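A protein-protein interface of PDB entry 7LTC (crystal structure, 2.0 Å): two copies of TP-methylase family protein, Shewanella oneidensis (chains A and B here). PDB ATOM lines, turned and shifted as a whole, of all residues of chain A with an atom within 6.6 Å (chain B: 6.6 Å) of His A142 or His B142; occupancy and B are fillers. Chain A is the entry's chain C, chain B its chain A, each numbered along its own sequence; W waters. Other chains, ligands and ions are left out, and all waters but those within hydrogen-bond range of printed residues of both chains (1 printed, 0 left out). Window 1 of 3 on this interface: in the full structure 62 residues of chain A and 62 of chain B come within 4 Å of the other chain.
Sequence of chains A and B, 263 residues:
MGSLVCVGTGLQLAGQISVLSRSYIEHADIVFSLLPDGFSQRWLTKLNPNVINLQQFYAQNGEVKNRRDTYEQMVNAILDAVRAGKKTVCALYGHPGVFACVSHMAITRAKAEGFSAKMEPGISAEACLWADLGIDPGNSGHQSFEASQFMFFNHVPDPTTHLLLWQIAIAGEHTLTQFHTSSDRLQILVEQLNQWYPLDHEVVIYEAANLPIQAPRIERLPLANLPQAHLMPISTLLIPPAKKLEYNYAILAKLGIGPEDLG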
ATOM      1  N   PHE A  99      29.739  11.386   9.710  1.00  0.00           N
ATOM      2  CA  PHE A  99      28.873  11.473   8.520  1.00  0.00           C
ATOM      3  C   PHE A  99      29.144  12.798   7.793  1.00  0.00           C
ATOM      4  O   PHE A  99      28.235  13.552   7.450  1.00  0.00           O
ATOM      5  CB  PHE A  99      27.410  11.243   8.917  1.00  0.00           C
ATOM      6  CG  PHE A  99      27.070   9.798   9.194  1.00  0.00           C
ATOM      7  CD1 PHE A  99      27.306   9.230  10.439  1.00  0.00           C
ATOM      8  CD2 PHE A  99      26.516   8.999   8.204  1.00  0.00           C
ATOM      9  CE1 PHE A  99      27.004   7.897  10.680  1.00  0.00           C
ATOM     10  CE2 PHE A  99      26.205   7.671   8.450  1.00  0.00           C
ATOM     11  CZ  PHE A  99      26.456   7.118   9.686  1.00  0.00           C
ATOM     12  N   GLU A 126      24.128  12.175  16.977  1.00  0.00           N
ATOM     13  CA  GLU A 126      23.935  10.932  17.716  1.00  0.00           C
ATOM     14  C   GLU A 126      24.265  11.176  19.198  1.00  0.00           C
ATOM     15  O   GLU A 126      23.572  10.664  20.074  1.00  0.00           O
ATOM     16  CB  GLU A 126      24.736   9.824  17.023  1.00  0.00           C
ATOM     17  CG  GLU A 126      25.452   8.849  17.934  1.00  0.00           C
ATOM     18  CD  GLU A 126      26.404   7.943  17.170  1.00  0.00           C
ATOM     19  OE1 GLU A 126      26.104   7.631  15.998  1.00  0.00           O
ATOM     20  OE2 GLU A 126      27.445   7.560  17.740  1.00  0.00           O
ATOM     21  N   TRP A 130      21.430  10.410  22.319  1.00  0.00           N
ATOM     22  CA  TRP A 130      21.547   9.582  23.540  1.00  0.00           C
ATOM     23  C   TRP A 130      21.046  10.388  24.746  1.00  0.00           C
ATOM     24  O   TRP A 130      20.360   9.857  25.620  1.00  0.00           O
ATOM     25  CB  TRP A 130      22.977   9.060  23.775  1.00  0.00           C
ATOM     26  CG  TRP A 130      23.599   8.345  22.613  1.00  0.00           C
ATOM     27  CD1 TRP A 130      24.824   8.602  22.069  1.00  0.00           C
ATOM     28  CD2 TRP A 130      23.050   7.248  21.854  1.00  0.00           C
ATOM     29  NE1 TRP A 130      25.070   7.758  21.022  1.00  0.00           N
ATOM     30  CE2 TRP A 130      24.001   6.918  20.862  1.00  0.00           C
ATOM     31  CE3 TRP A 130      21.854   6.522  21.898  1.00  0.00           C
ATOM     32  CZ2 TRP A 130      23.795   5.896  19.937  1.00  0.00           C
ATOM     33  CZ3 TRP A 130      21.652   5.510  20.984  1.00  0.00           C
ATOM     34  CH2 TRP A 130      22.611   5.202  20.017  1.00  0.00           C
ATOM     35  N   ASP A 136      21.591   4.806  26.683  1.00  0.00           N
ATOM     36  CA  ASP A 136      23.047   4.552  26.624  1.00  0.00           C
ATOM     37  C   ASP A 136      23.342   3.572  25.478  1.00  0.00           C
ATOM     38  O   ASP A 136      22.809   2.469  25.476  1.00  0.00           O
ATOM     39  CB  ASP A 136      23.558   3.975  27.948  1.00  0.00           C
ATOM     40  CG  ASP A 136      25.066   3.800  28.053  1.00  0.00           C
ATOM     41  OD1 ASP A 136      25.741   3.780  26.999  1.00  0.00           O
ATOM     42  OD2 ASP A 136      25.554   3.669  29.196  1.00  0.00           O
ATOM     43  N   PRO A 137      24.195   3.959  24.504  1.00  0.00           N
ATOM     44  CA  PRO A 137      24.518   3.038  23.403  1.00  0.00           C
ATOM     45  C   PRO A 137      25.197   1.750  23.896  1.00  0.00           C
ATOM     46  O   PRO A 137      25.229   0.760  23.164  1.00  0.00           O
ATOM     47  CB  PRO A 137      25.461   3.814  22.469  1.00  0.00           C
ATOM     48  CG  PRO A 137      26.017   4.897  23.353  1.00  0.00           C
ATOM     49  CD  PRO A 137      24.849   5.248  24.249  1.00  0.00           C
ATOM     50  N   GLY A 138      25.721   1.760  25.118  1.00  0.00           N
ATOM     51  CA  GLY A 138      26.351   0.563  25.687  1.00  0.00           C
ATOM     52  C   GLY A 138      25.346  -0.405  26.297  1.00  0.00           C
ATOM     53  O   GLY A 138      25.701  -1.540  26.622  1.00  0.00           O
ATOM     54  N   SER A 140      22.646  -2.112  25.207  1.00  0.00           N
ATOM     55  CA  SER A 140      22.645  -3.357  24.440  1.00  0.00           C
ATOM     56  C   SER A 140      23.452  -3.173  23.150  1.00  0.00           C
ATOM     57  O   SER A 140      23.341  -3.986  22.236  1.00  0.00           O
ATOM     58  CB  SER A 140      21.248  -3.848  24.149  1.00  0.00           C
ATOM     59  OG  SER A 140      20.469  -2.834  23.535  1.00  0.00           O
ATOM     60  N   GLY A 141      24.262  -2.116  23.091  1.00  0.00           N
ATOM     61  CA  GLY A 141      25.160  -1.877  21.947  1.00  0.00           C
ATOM     62  C   GLY A 141      24.502  -1.032  20.868  1.00  0.00           C
ATOM     63  O   GLY A 141      23.297  -0.790  20.908  1.00  0.00           O
ATOM     64  N   HIS A 142      25.282  -0.587  19.887  1.00  0.00           N
ATOM     65  CA  HIS A 142      24.760   0.366  18.907  1.00  0.00           C
ATOM     66  C   HIS A 142      25.357   0.108  17.517  1.00  0.00           C
ATOM     67  O   HIS A 142      26.476  -0.380  17.393  1.00  0.00           O
ATOM     68  CB  HIS A 142      24.982   1.779  19.465  1.00  0.00           C
ATOM     69  CG  HIS A 142      25.347   2.837  18.484  1.00  0.00           C
ATOM     70  ND1 HIS A 142      26.555   3.494  18.550  1.00  0.00           N
ATOM     71  CD2 HIS A 142      24.652   3.416  17.481  1.00  0.00           C
ATOM     72  CE1 HIS A 142      26.608   4.408  17.606  1.00  0.00           C
ATOM     73  NE2 HIS A 142      25.455   4.378  16.935  1.00  0.00           N
ATOM     74  N   GLN A 143      24.563   0.411  16.487  1.00  0.00           N
ATOM     75  CA  GLN A 143      24.970   0.311  15.078  1.00  0.00           C
ATOM     76  C   GLN A 143      24.471   1.538  14.310  1.00  0.00           C
ATOM     77  O   GLN A 143      23.339   1.990  14.502  1.00  0.00           O
ATOM     78  CB  GLN A 143      24.366  -0.916  14.401  1.00  0.00           C
ATOM     79  CG  GLN A 143      24.624  -2.213  15.134  1.00  0.00           C
ATOM     80  CD  GLN A 143      23.911  -3.315  14.395  1.00  0.00           C
ATOM     81  OE1 GLN A 143      24.485  -3.981  13.526  1.00  0.00           O
ATOM     82  NE2 GLN A 143      22.630  -3.466  14.685  1.00  0.00           N
ATOM     83  N   SER A 144      25.307   2.032  13.408  1.00  0.00           N
ATOM     84  CA  SER A 144      25.007   3.220  12.619  1.00  0.00           C
ATOM     85  C   SER A 144      25.305   2.944  11.143  1.00  0.00           C
ATOM     86  O   SER A 144      26.389   2.476  10.825  1.00  0.00           O
ATOM     87  CB  SER A 144      25.831   4.388  13.088  1.00  0.00           C
ATOM     88  OG  SER A 144      25.128   5.175  14.038  1.00  0.00           O
ATOM     89  N   PHE A 145      24.365   3.242  10.257  1.00  0.00           N
ATOM     90  CA  PHE A 145      24.656   3.202   8.832  1.00  0.00           C
ATOM     91  C   PHE A 145      24.001   4.393   8.139  1.00  0.00           C
ATOM     92  O   PHE A 145      22.966   4.880   8.575  1.00  0.00           O
ATOM     93  CB  PHE A 145      24.074   1.971   8.134  1.00  0.00           C
ATOM     94  CG  PHE A 145      24.420   0.644   8.751  1.00  0.00           C
ATOM     95  CD1 PHE A 145      25.582  -0.023   8.400  1.00  0.00           C
ATOM     96  CD2 PHE A 145      23.568   0.053   9.665  1.00  0.00           C
ATOM     97  CE1 PHE A 145      25.892  -1.250   8.966  1.00  0.00           C
ATOM     98  CE2 PHE A 145      23.880  -1.173  10.232  1.00  0.00           C
ATOM     99  CZ  PHE A 145      25.040  -1.822   9.882  1.00  0.00           C
ATOM    100  N   THR A 161      20.499  -4.590  19.282  1.00  0.00           N
ATOM    101  CA  THR A 161      21.148  -3.292  19.497  1.00  0.00           C
ATOM    102  C   THR A 161      20.212  -2.144  19.115  1.00  0.00           C
ATOM    103  O   THR A 161      19.199  -2.351  18.450  1.00  0.00           O
ATOM    104  CB  THR A 161      22.406  -3.136  18.637  1.00  0.00           C
ATOM    105  OG1 THR A 161      21.952  -2.976  17.287  1.00  0.00           O
ATOM    106  CG2 THR A 161      23.363  -4.302  18.753  1.00  0.00           C
ATOM    107  N   HIS A 162      20.580  -0.932  19.521  1.00  0.00           N
ATOM    108  CA  HIS A 162      19.944   0.259  18.984  1.00  0.00           C
ATOM    109  C   HIS A 162      20.525   0.557  17.602  1.00  0.00           C
ATOM    110  O   HIS A 162      21.727   0.788  17.464  1.00  0.00           O
ATOM    111  CB  HIS A 162      20.123   1.456  19.922  1.00  0.00           C
ATOM    112  CG  HIS A 162      19.149   1.449  21.047  1.00  0.00           C
ATOM    113  ND1 HIS A 162      19.427   0.838  22.252  1.00  0.00           N
ATOM    114  CD2 HIS A 162      17.894   1.937  21.138  1.00  0.00           C
ATOM    115  CE1 HIS A 162      18.386   0.961  23.049  1.00  0.00           C
ATOM    116  NE2 HIS A 162      17.430   1.631  22.387  1.00  0.00           N
ATOM    117  N   LEU A 163      19.664   0.579  16.594  1.00  0.00           N
ATOM    118  CA  LEU A 163      20.122   0.773  15.224  1.00  0.00           C
ATOM    119  C   LEU A 163      19.735   2.181  14.740  1.00  0.00           C
ATOM    120  O   LEU A 163      18.581   2.604  14.855  1.00  0.00           O
ATOM    121  CB  LEU A 163      19.496  -0.327  14.359  1.00  0.00           C
ATOM    122  CG  LEU A 163      19.560  -0.120  12.850  1.00  0.00           C
ATOM    123  CD1 LEU A 163      20.982  -0.277  12.346  1.00  0.00           C
ATOM    124  CD2 LEU A 163      18.643  -1.101  12.141  1.00  0.00           C
ATOM    125  N   LEU A 164      20.704   2.899  14.187  1.00  0.00           N
ATOM    126  CA  LEU A 164      20.463   4.243  13.662  1.00  0.00           C
ATOM    127  C   LEU A 164      20.660   4.241  12.141  1.00  0.00           C
ATOM    128  O   LEU A 164      21.718   3.848  11.658  1.00  0.00           O
ATOM    129  CB  LEU A 164      21.441   5.229  14.315  1.00  0.00           C
ATOM    130  CG  LEU A 164      21.171   5.623  15.767  1.00  0.00           C
ATOM    131  CD1 LEU A 164      22.279   6.529  16.276  1.00  0.00           C
ATOM    132  CD2 LEU A 164      19.838   6.338  15.902  1.00  0.00           C
ATOM    133  N   TRP A 166      21.029   6.973   9.358  1.00  0.00           N
ATOM    134  CA  TRP A 166      21.265   8.395   9.137  1.00  0.00           C
ATOM    135  C   TRP A 166      20.801   8.778   7.729  1.00  0.00           C
ATOM    136  O   TRP A 166      20.785   7.934   6.833  1.00  0.00           O
ATOM    137  CB  TRP A 166      22.754   8.709   9.282  1.00  0.00           C
ATOM    138  CG  TRP A 166      23.321   8.583  10.658  1.00  0.00           C
ATOM    139  CD1 TRP A 166      23.384   7.457  11.428  1.00  0.00           C
ATOM    140  CD2 TRP A 166      23.990   9.619  11.397  1.00  0.00           C
ATOM    141  NE1 TRP A 166      24.019   7.728  12.609  1.00  0.00           N
ATOM    142  CE2 TRP A 166      24.403   9.044  12.617  1.00  0.00           C
ATOM    143  CE3 TRP A 166      24.273  10.968  11.153  1.00  0.00           C
ATOM    144  CZ2 TRP A 166      25.086   9.776  13.589  1.00  0.00           C
ATOM    145  CZ3 TRP A 166      24.942  11.690  12.116  1.00  0.00           C
ATOM    146  CH2 TRP A 166      25.341  11.101  13.317  1.00  0.00           C
ATOM    147  N   PHE B  99      28.265   4.895  27.529  1.00  0.00           N
ATOM    148  CA  PHE B  99      28.946   3.858  28.327  1.00  0.00           C
ATOM    149  C   PHE B  99      29.110   4.390  29.756  1.00  0.00           C
ATOM    150  O   PHE B  99      30.190   4.363  30.344  1.00  0.00           O
ATOM    151  CB  PHE B  99      30.250   3.409  27.653  1.00  0.00           C
ATOM    152  CG  PHE B  99      30.049   2.486  26.473  1.00  0.00           C
ATOM    153  CD1 PHE B  99      29.802   2.998  25.208  1.00  0.00           C
ATOM    154  CD2 PHE B  99      30.087   1.108  26.627  1.00  0.00           C
ATOM    155  CE1 PHE B  99      29.595   2.157  24.123  1.00  0.00           C
ATOM    156  CE2 PHE B  99      29.883   0.268  25.541  1.00  0.00           C
ATOM    157  CZ  PHE B  99      29.636   0.793  24.291  1.00  0.00           C
ATOM    158  N   GLU B 126      34.758   7.778  21.647  1.00  0.00           N
ATOM    159  CA  GLU B 126      34.520   7.357  20.258  1.00  0.00           C
ATOM    160  C   GLU B 126      34.577   8.597  19.350  1.00  0.00           C
ATOM    161  O   GLU B 126      35.127   8.530  18.252  1.00  0.00           O
ATOM    162  CB  GLU B 126      33.230   6.526  20.219  1.00  0.00           C
ATOM    163  CG  GLU B 126      32.336   6.701  18.999  1.00  0.00           C
ATOM    164  CD  GLU B 126      31.024   5.937  19.101  1.00  0.00           C
ATOM    165  OE1 GLU B 126      31.054   4.770  19.546  1.00  0.00           O
ATOM    166  OE2 GLU B 126      29.973   6.509  18.744  1.00  0.00           O
ATOM    167  N   TRP B 130      37.384   8.909  16.049  1.00  0.00           N
ATOM    168  CA  TRP B 130      37.126   9.212  14.628  1.00  0.00           C
ATOM    169  C   TRP B 130      38.077  10.327  14.162  1.00  0.00           C
ATOM    170  O   TRP B 130      38.614  10.273  13.051  1.00  0.00           O
ATOM    171  CB  TRP B 130      35.658   9.593  14.370  1.00  0.00           C
ATOM    172  CG  TRP B 130      34.637   8.635  14.906  1.00  0.00           C
ATOM    173  CD1 TRP B 130      33.578   8.959  15.702  1.00  0.00           C
ATOM    174  CD2 TRP B 130      34.545   7.217  14.678  1.00  0.00           C
ATOM    175  NE1 TRP B 130      32.849   7.844  16.005  1.00  0.00           N
ATOM    176  CE2 TRP B 130      33.412   6.761  15.386  1.00  0.00           C
ATOM    177  CE3 TRP B 130      35.306   6.287  13.965  1.00  0.00           C
ATOM    178  CZ2 TRP B 130      33.020   5.426  15.399  1.00  0.00           C
ATOM    179  CZ3 TRP B 130      34.919   4.965  13.978  1.00  0.00           C
ATOM    180  CH2 TRP B 130      33.791   4.542  14.683  1.00  0.00           C
ATOM    181  N   ASP B 136      35.579   8.000   9.356  1.00  0.00           N
ATOM    182  CA  ASP B 136      34.181   8.414   9.461  1.00  0.00           C
ATOM    183  C   ASP B 136      33.328   7.163   9.695  1.00  0.00           C
ATOM    184  O   ASP B 136      33.393   6.212   8.916  1.00  0.00           O
ATOM    185  CB  ASP B 136      33.746   9.168   8.202  1.00  0.00           C
ATOM    186  CG  ASP B 136      32.334   9.732   8.210  1.00  0.00           C
ATOM    187  OD1 ASP B 136      31.502   9.273   9.032  1.00  0.00           O
ATOM    188  OD2 ASP B 136      32.067  10.620   7.364  1.00  0.00           O
ATOM    189  N   PRO B 137      32.540   7.144  10.775  1.00  0.00           N
ATOM    190  CA  PRO B 137      31.731   5.945  11.008  1.00  0.00           C
ATOM    191  C   PRO B 137      30.728   5.692   9.869  1.00  0.00           C
ATOM    192  O   PRO B 137      30.246   4.570   9.714  1.00  0.00           O
ATOM    193  CB  PRO B 137      31.016   6.225  12.339  1.00  0.00           C
ATOM    194  CG  PRO B 137      30.997   7.723  12.408  1.00  0.00           C
ATOM    195  CD  PRO B 137      32.363   8.095  11.877  1.00  0.00           C
ATOM    196  N   GLY B 138      30.417   6.727   9.081  1.00  0.00           N
ATOM    197  CA  GLY B 138      29.493   6.601   7.934  1.00  0.00           C
ATOM    198  C   GLY B 138      30.130   5.930   6.724  1.00  0.00           C
ATOM    199  O   GLY B 138      29.416   5.557   5.794  1.00  0.00           O
ATOM    200  N   SER B 140      31.662   2.983   6.046  1.00  0.00           N
ATOM    201  CA  SER B 140      31.105   1.652   5.808  1.00  0.00           C
ATOM    202  C   SER B 140      30.225   1.234   6.992  1.00  0.00           C
ATOM    203  O   SER B 140      29.902   0.056   7.142  1.00  0.00           O
ATOM    204  CB  SER B 140      32.188   0.632   5.553  1.00  0.00           C
ATOM    205  OG  SER B 140      33.130   0.603   6.618  1.00  0.00           O
ATOM    206  N   GLY B 141      29.853   2.196   7.827  1.00  0.00           N
ATOM    207  CA  GLY B 141      29.067   1.911   9.026  1.00  0.00           C
ATOM    208  C   GLY B 141      29.935   1.643  10.244  1.00  0.00           C
ATOM    209  O   GLY B 141      31.156   1.468  10.143  1.00  0.00           O
ATOM    210  N   HIS B 142      29.263   1.601  11.395  1.00  0.00           N
ATOM    211  CA  HIS B 142      29.907   1.506  12.696  1.00  0.00           C
ATOM    212  C   HIS B 142      29.047   0.663  13.653  1.00  0.00           C
ATOM    213  O   HIS B 142      27.827   0.781  13.668  1.00  0.00           O
ATOM    214  CB  HIS B 142      30.166   2.933  13.195  1.00  0.00           C
ATOM    215  CG  HIS B 142      30.167   3.097  14.672  1.00  0.00           C
ATOM    216  ND1 HIS B 142      29.418   4.072  15.294  1.00  0.00           N
ATOM    217  CD2 HIS B 142      30.829   2.437  15.643  1.00  0.00           C
ATOM    218  CE1 HIS B 142      29.623   4.012  16.594  1.00  0.00           C
ATOM    219  NE2 HIS B 142      30.477   3.008  16.834  1.00  0.00           N
ATOM    220  N   GLN B 143      29.687  -0.200  14.437  1.00  0.00           N
ATOM    221  CA  GLN B 143      29.010  -0.900  15.532  1.00  0.00           C
ATOM    222  C   GLN B 143      29.856  -0.773  16.806  1.00  0.00           C
ATOM    223  O   GLN B 143      31.087  -0.828  16.742  1.00  0.00           O
ATOM    224  CB  GLN B 143      28.842  -2.394  15.245  1.00  0.00           C
ATOM    225  CG  GLN B 143      28.143  -2.744  13.943  1.00  0.00           C
ATOM    226  CD  GLN B 143      28.290  -4.221  13.663  1.00  0.00           C
ATOM    227  OE1 GLN B 143      27.326  -4.984  13.701  1.00  0.00           O
ATOM    228  NE2 GLN B 143      29.519  -4.643  13.405  1.00  0.00           N
ATOM    229  N   SER B 144      29.184  -0.635  17.949  1.00  0.00           N
ATOM    230  CA  SER B 144      29.818  -0.566  19.273  1.00  0.00           C
ATOM    231  C   SER B 144      29.153  -1.571  20.216  1.00  0.00           C
ATOM    232  O   SER B 144      27.929  -1.625  20.300  1.00  0.00           O
ATOM    233  CB  SER B 144      29.715   0.816  19.880  1.00  0.00           C
ATOM    234  OG  SER B 144      30.665   1.703  19.314  1.00  0.00           O
ATOM    235  N   PHE B 145      29.970  -2.299  20.961  1.00  0.00           N
ATOM    236  CA  PHE B 145      29.512  -3.140  22.043  1.00  0.00           C
ATOM    237  C   PHE B 145      30.509  -3.069  23.195  1.00  0.00           C
ATOM    238  O   PHE B 145      31.704  -2.883  22.963  1.00  0.00           O
ATOM    239  CB  PHE B 145      29.516  -4.615  21.659  1.00  0.00           C
ATOM    240  CG  PHE B 145      28.738  -4.936  20.419  1.00  0.00           C
ATOM    241  CD1 PHE B 145      27.375  -5.167  20.488  1.00  0.00           C
ATOM    242  CD2 PHE B 145      29.371  -4.999  19.191  1.00  0.00           C
ATOM    243  CE1 PHE B 145      26.661  -5.481  19.346  1.00  0.00           C
ATOM    244  CE2 PHE B 145      28.655  -5.319  18.051  1.00  0.00           C
ATOM    245  CZ  PHE B 145      27.301  -5.548  18.130  1.00  0.00           C
ATOM    246  N   THR B 161      31.777  -3.195   8.616  1.00  0.00           N
ATOM    247  CA  THR B 161      31.768  -1.954   9.405  1.00  0.00           C
ATOM    248  C   THR B 161      33.067  -1.796  10.200  1.00  0.00           C
ATOM    249  O   THR B 161      33.869  -2.721  10.286  1.00  0.00           O
ATOM    250  CB  THR B 161      30.606  -1.912  10.403  1.00  0.00           C
ATOM    251  OG1 THR B 161      30.846  -2.902  11.406  1.00  0.00           O
ATOM    252  CG2 THR B 161      29.264  -2.132   9.741  1.00  0.00           C
ATOM    253  N   HIS B 162      33.250  -0.611  10.777  1.00  0.00           N
ATOM    254  CA  HIS B 162      34.202  -0.451  11.857  1.00  0.00           C
ATOM    255  C   HIS B 162      33.522  -0.902  13.153  1.00  0.00           C
ATOM    256  O   HIS B 162      32.465  -0.387  13.514  1.00  0.00           O
ATOM    257  CB  HIS B 162      34.712   0.992  11.936  1.00  0.00           C
ATOM    258  CG  HIS B 162      35.615   1.348  10.804  1.00  0.00           C
ATOM    259  ND1 HIS B 162      36.986   1.210  10.883  1.00  0.00           N
ATOM    260  CD2 HIS B 162      35.350   1.813   9.565  1.00  0.00           C
ATOM    261  CE1 HIS B 162      37.530   1.583   9.743  1.00  0.00           C
ATOM    262  NE2 HIS B 162      36.547   1.957   8.915  1.00  0.00           N
ATOM    263  N   LEU B 163      34.119  -1.885  13.813  1.00  0.00           N
ATOM    264  CA  LEU B 163      33.565  -2.468  15.041  1.00  0.00           C
ATOM    265  C   LEU B 163      34.402  -2.011  16.244  1.00  0.00           C
ATOM    266  O   LEU B 163      35.635  -2.118  16.220  1.00  0.00           O
ATOM    267  CB  LEU B 163      33.573  -3.995  14.879  1.00  0.00           C
ATOM    268  CG  LEU B 163      33.352  -4.846  16.131  1.00  0.00           C
ATOM    269  CD1 LEU B 163      31.963  -4.629  16.702  1.00  0.00           C
ATOM    270  CD2 LEU B 163      33.550  -6.324  15.813  1.00  0.00           C
ATOM    271  N   LEU B 164      33.734  -1.491  17.279  1.00  0.00           N
ATOM    272  CA  LEU B 164      34.402  -1.051  18.518  1.00  0.00           C
ATOM    273  C   LEU B 164      33.997  -1.980  19.671  1.00  0.00           C
ATOM    274  O   LEU B 164      32.815  -2.177  19.922  1.00  0.00           O
ATOM    275  CB  LEU B 164      33.997   0.395  18.844  1.00  0.00           C
ATOM    276  CG  LEU B 164      34.586   1.499  17.963  1.00  0.00           C
ATOM    277  CD1 LEU B 164      34.124   2.869  18.439  1.00  0.00           C
ATOM    278  CD2 LEU B 164      36.104   1.454  17.950  1.00  0.00           C
ATOM    279  N   TRP B 166      34.369  -1.772  23.546  1.00  0.00           N
ATOM    280  CA  TRP B 166      34.709  -0.892  24.656  1.00  0.00           C
ATOM    281  C   TRP B 166      35.026  -1.747  25.892  1.00  0.00           C
ATOM    282  O   TRP B 166      34.544  -2.872  26.018  1.00  0.00           O
ATOM    283  CB  TRP B 166      33.552   0.068  24.970  1.00  0.00           C
ATOM    284  CG  TRP B 166      33.184   1.091  23.940  1.00  0.00           C
ATOM    285  CD1 TRP B 166      32.765   0.872  22.659  1.00  0.00           C
ATOM    286  CD2 TRP B 166      33.096   2.514  24.155  1.00  0.00           C
ATOM    287  NE1 TRP B 166      32.465   2.062  22.049  1.00  0.00           N
ATOM    288  CE2 TRP B 166      32.656   3.087  22.943  1.00  0.00           C
ATOM    289  CE3 TRP B 166      33.363   3.359  25.242  1.00  0.00           C
ATOM    290  CZ2 TRP B 166      32.478   4.466  22.795  1.00  0.00           C
ATOM    291  CZ3 TRP B 166      33.184   4.719  25.094  1.00  0.00           C
ATOM    292  CH2 TRP B 166      32.748   5.263  23.885  1.00  0.00           C
HETATM  293  O   HOH W   1      28.005   6.342  14.648  1.00  0.00           O
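Phe A99 touches Asp B136, and with the chains exchanged Asp A136 touches Phe B99.
Phe A99 touches Gly B138, and with the chains exchanged Gly A138 touches Phe B99.
Gly A141 touches Ser B144, and with the chains exchanged Ser A144 touches Gly B141.
His A142 touches its own counterpart, His B142.
O of Gly A141 is in hydrogen-bond range of N of His A162, 3.1 Å away.
N of Gln A143 sits at hydrogen-bond distance from O of His A162 (3.0 Å).
The side-chain hydroxyl (OG) of Ser A144 is in hydrogen-bond range of the side-chain carboxylate (OE1) of Glu A126, at 3.3 Å.
NE1 of Trp A166 sits at hydrogen-bond distance from OG of Ser A144.
The backbone carbonyl oxygen (O) of Gly B141 sits at hydrogen-bond distance from the backbone NH (N) of His B162 (3.0 Å).
The side-chain carboxylate of Asp B136 is in hydrogen-bond range of the backbone NH of Gly B138 (2.8 Å).
Water W1 lies within hydrogen-bond range of OE1 of Glu A126 (2.7 Å), ND1 of His B142 (2.8 Å) and OG of Ser A144 (3.2 Å).
Hydrophobic or aromatic side chains of chain A within 4 Å of the printed part of chain B: Phe A99, His A142 and Phe A145.
Among the printed residues, 15 pairs touch across the chains.
Among the printed residues, no Asp or Glu carboxylate lies within 4 Å of a Lys or Arg side-chain nitrogen of the other chain.
Printed residues of chain B within 4 Å of Glu A126: Glu B126 (2.9 Å).
Trp A130 touches none of the printed residues of chain B.
Pro A137 touches none of the printed residues of chain B.
His A142 touches just these residues of chain B: His B142 (3.2 Å), Gln B143 (3.2 Å) and Ser B144 (2.8 Å).
Of the printed residues of chain A, Glu B126 touches Glu A126.
His B142 touches just these residues of chain A: His A142 (3.2 Å), Gln A143 (3.2 Å) and Ser A144 (2.8 Å).
The nearest residue of chain B that does not touch His A142 is Glu B126 (4.1 Å).
The nearest residue of chain A that does not touch His B142 is Glu A126 (4.3 Å).
Among the printed residues, pairs that only touch across the chains: His A142 with Gln B143 (3.2 Å), His A142 with His B142 (3.2 Å), Gln A143 with His B142 (3.2 Å), Gly A141 with Ser B144 (3.2 Å), Ser A144 with Gly B141 (3.3 Å), Phe A99 with Gly B138 (3.5 Å), Gly A138 with Phe B99 (3.5 Å), Thr A161 with Phe B145 (3.6 Å) and Phe A145 with Thr B161 (3.6 Å).
The backbone carbonyl oxygen (O) of His B142 sits at hydrogen-bond distance from the backbone NH (N) of Ser A144 (2.8 Å).
OD1 of Asp A136 sits at hydrogen-bond distance from N of Phe B99, 2.8 Å away.
The side-chain carboxylate (OD1) of Asp B136 sits at hydrogen-bond distance from the backbone NH (N) of Phe A99 (2.8 Å).
N of Ser B144 lies within hydrogen-bond range of O of His A142, at 2.8 Å.
OE2 of Glu A126 sits close to OE2 of Glu B126 (2.9 Å).
OE1 of Gln A143 sits close to OE1 of Gln B143 (3.0 Å).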
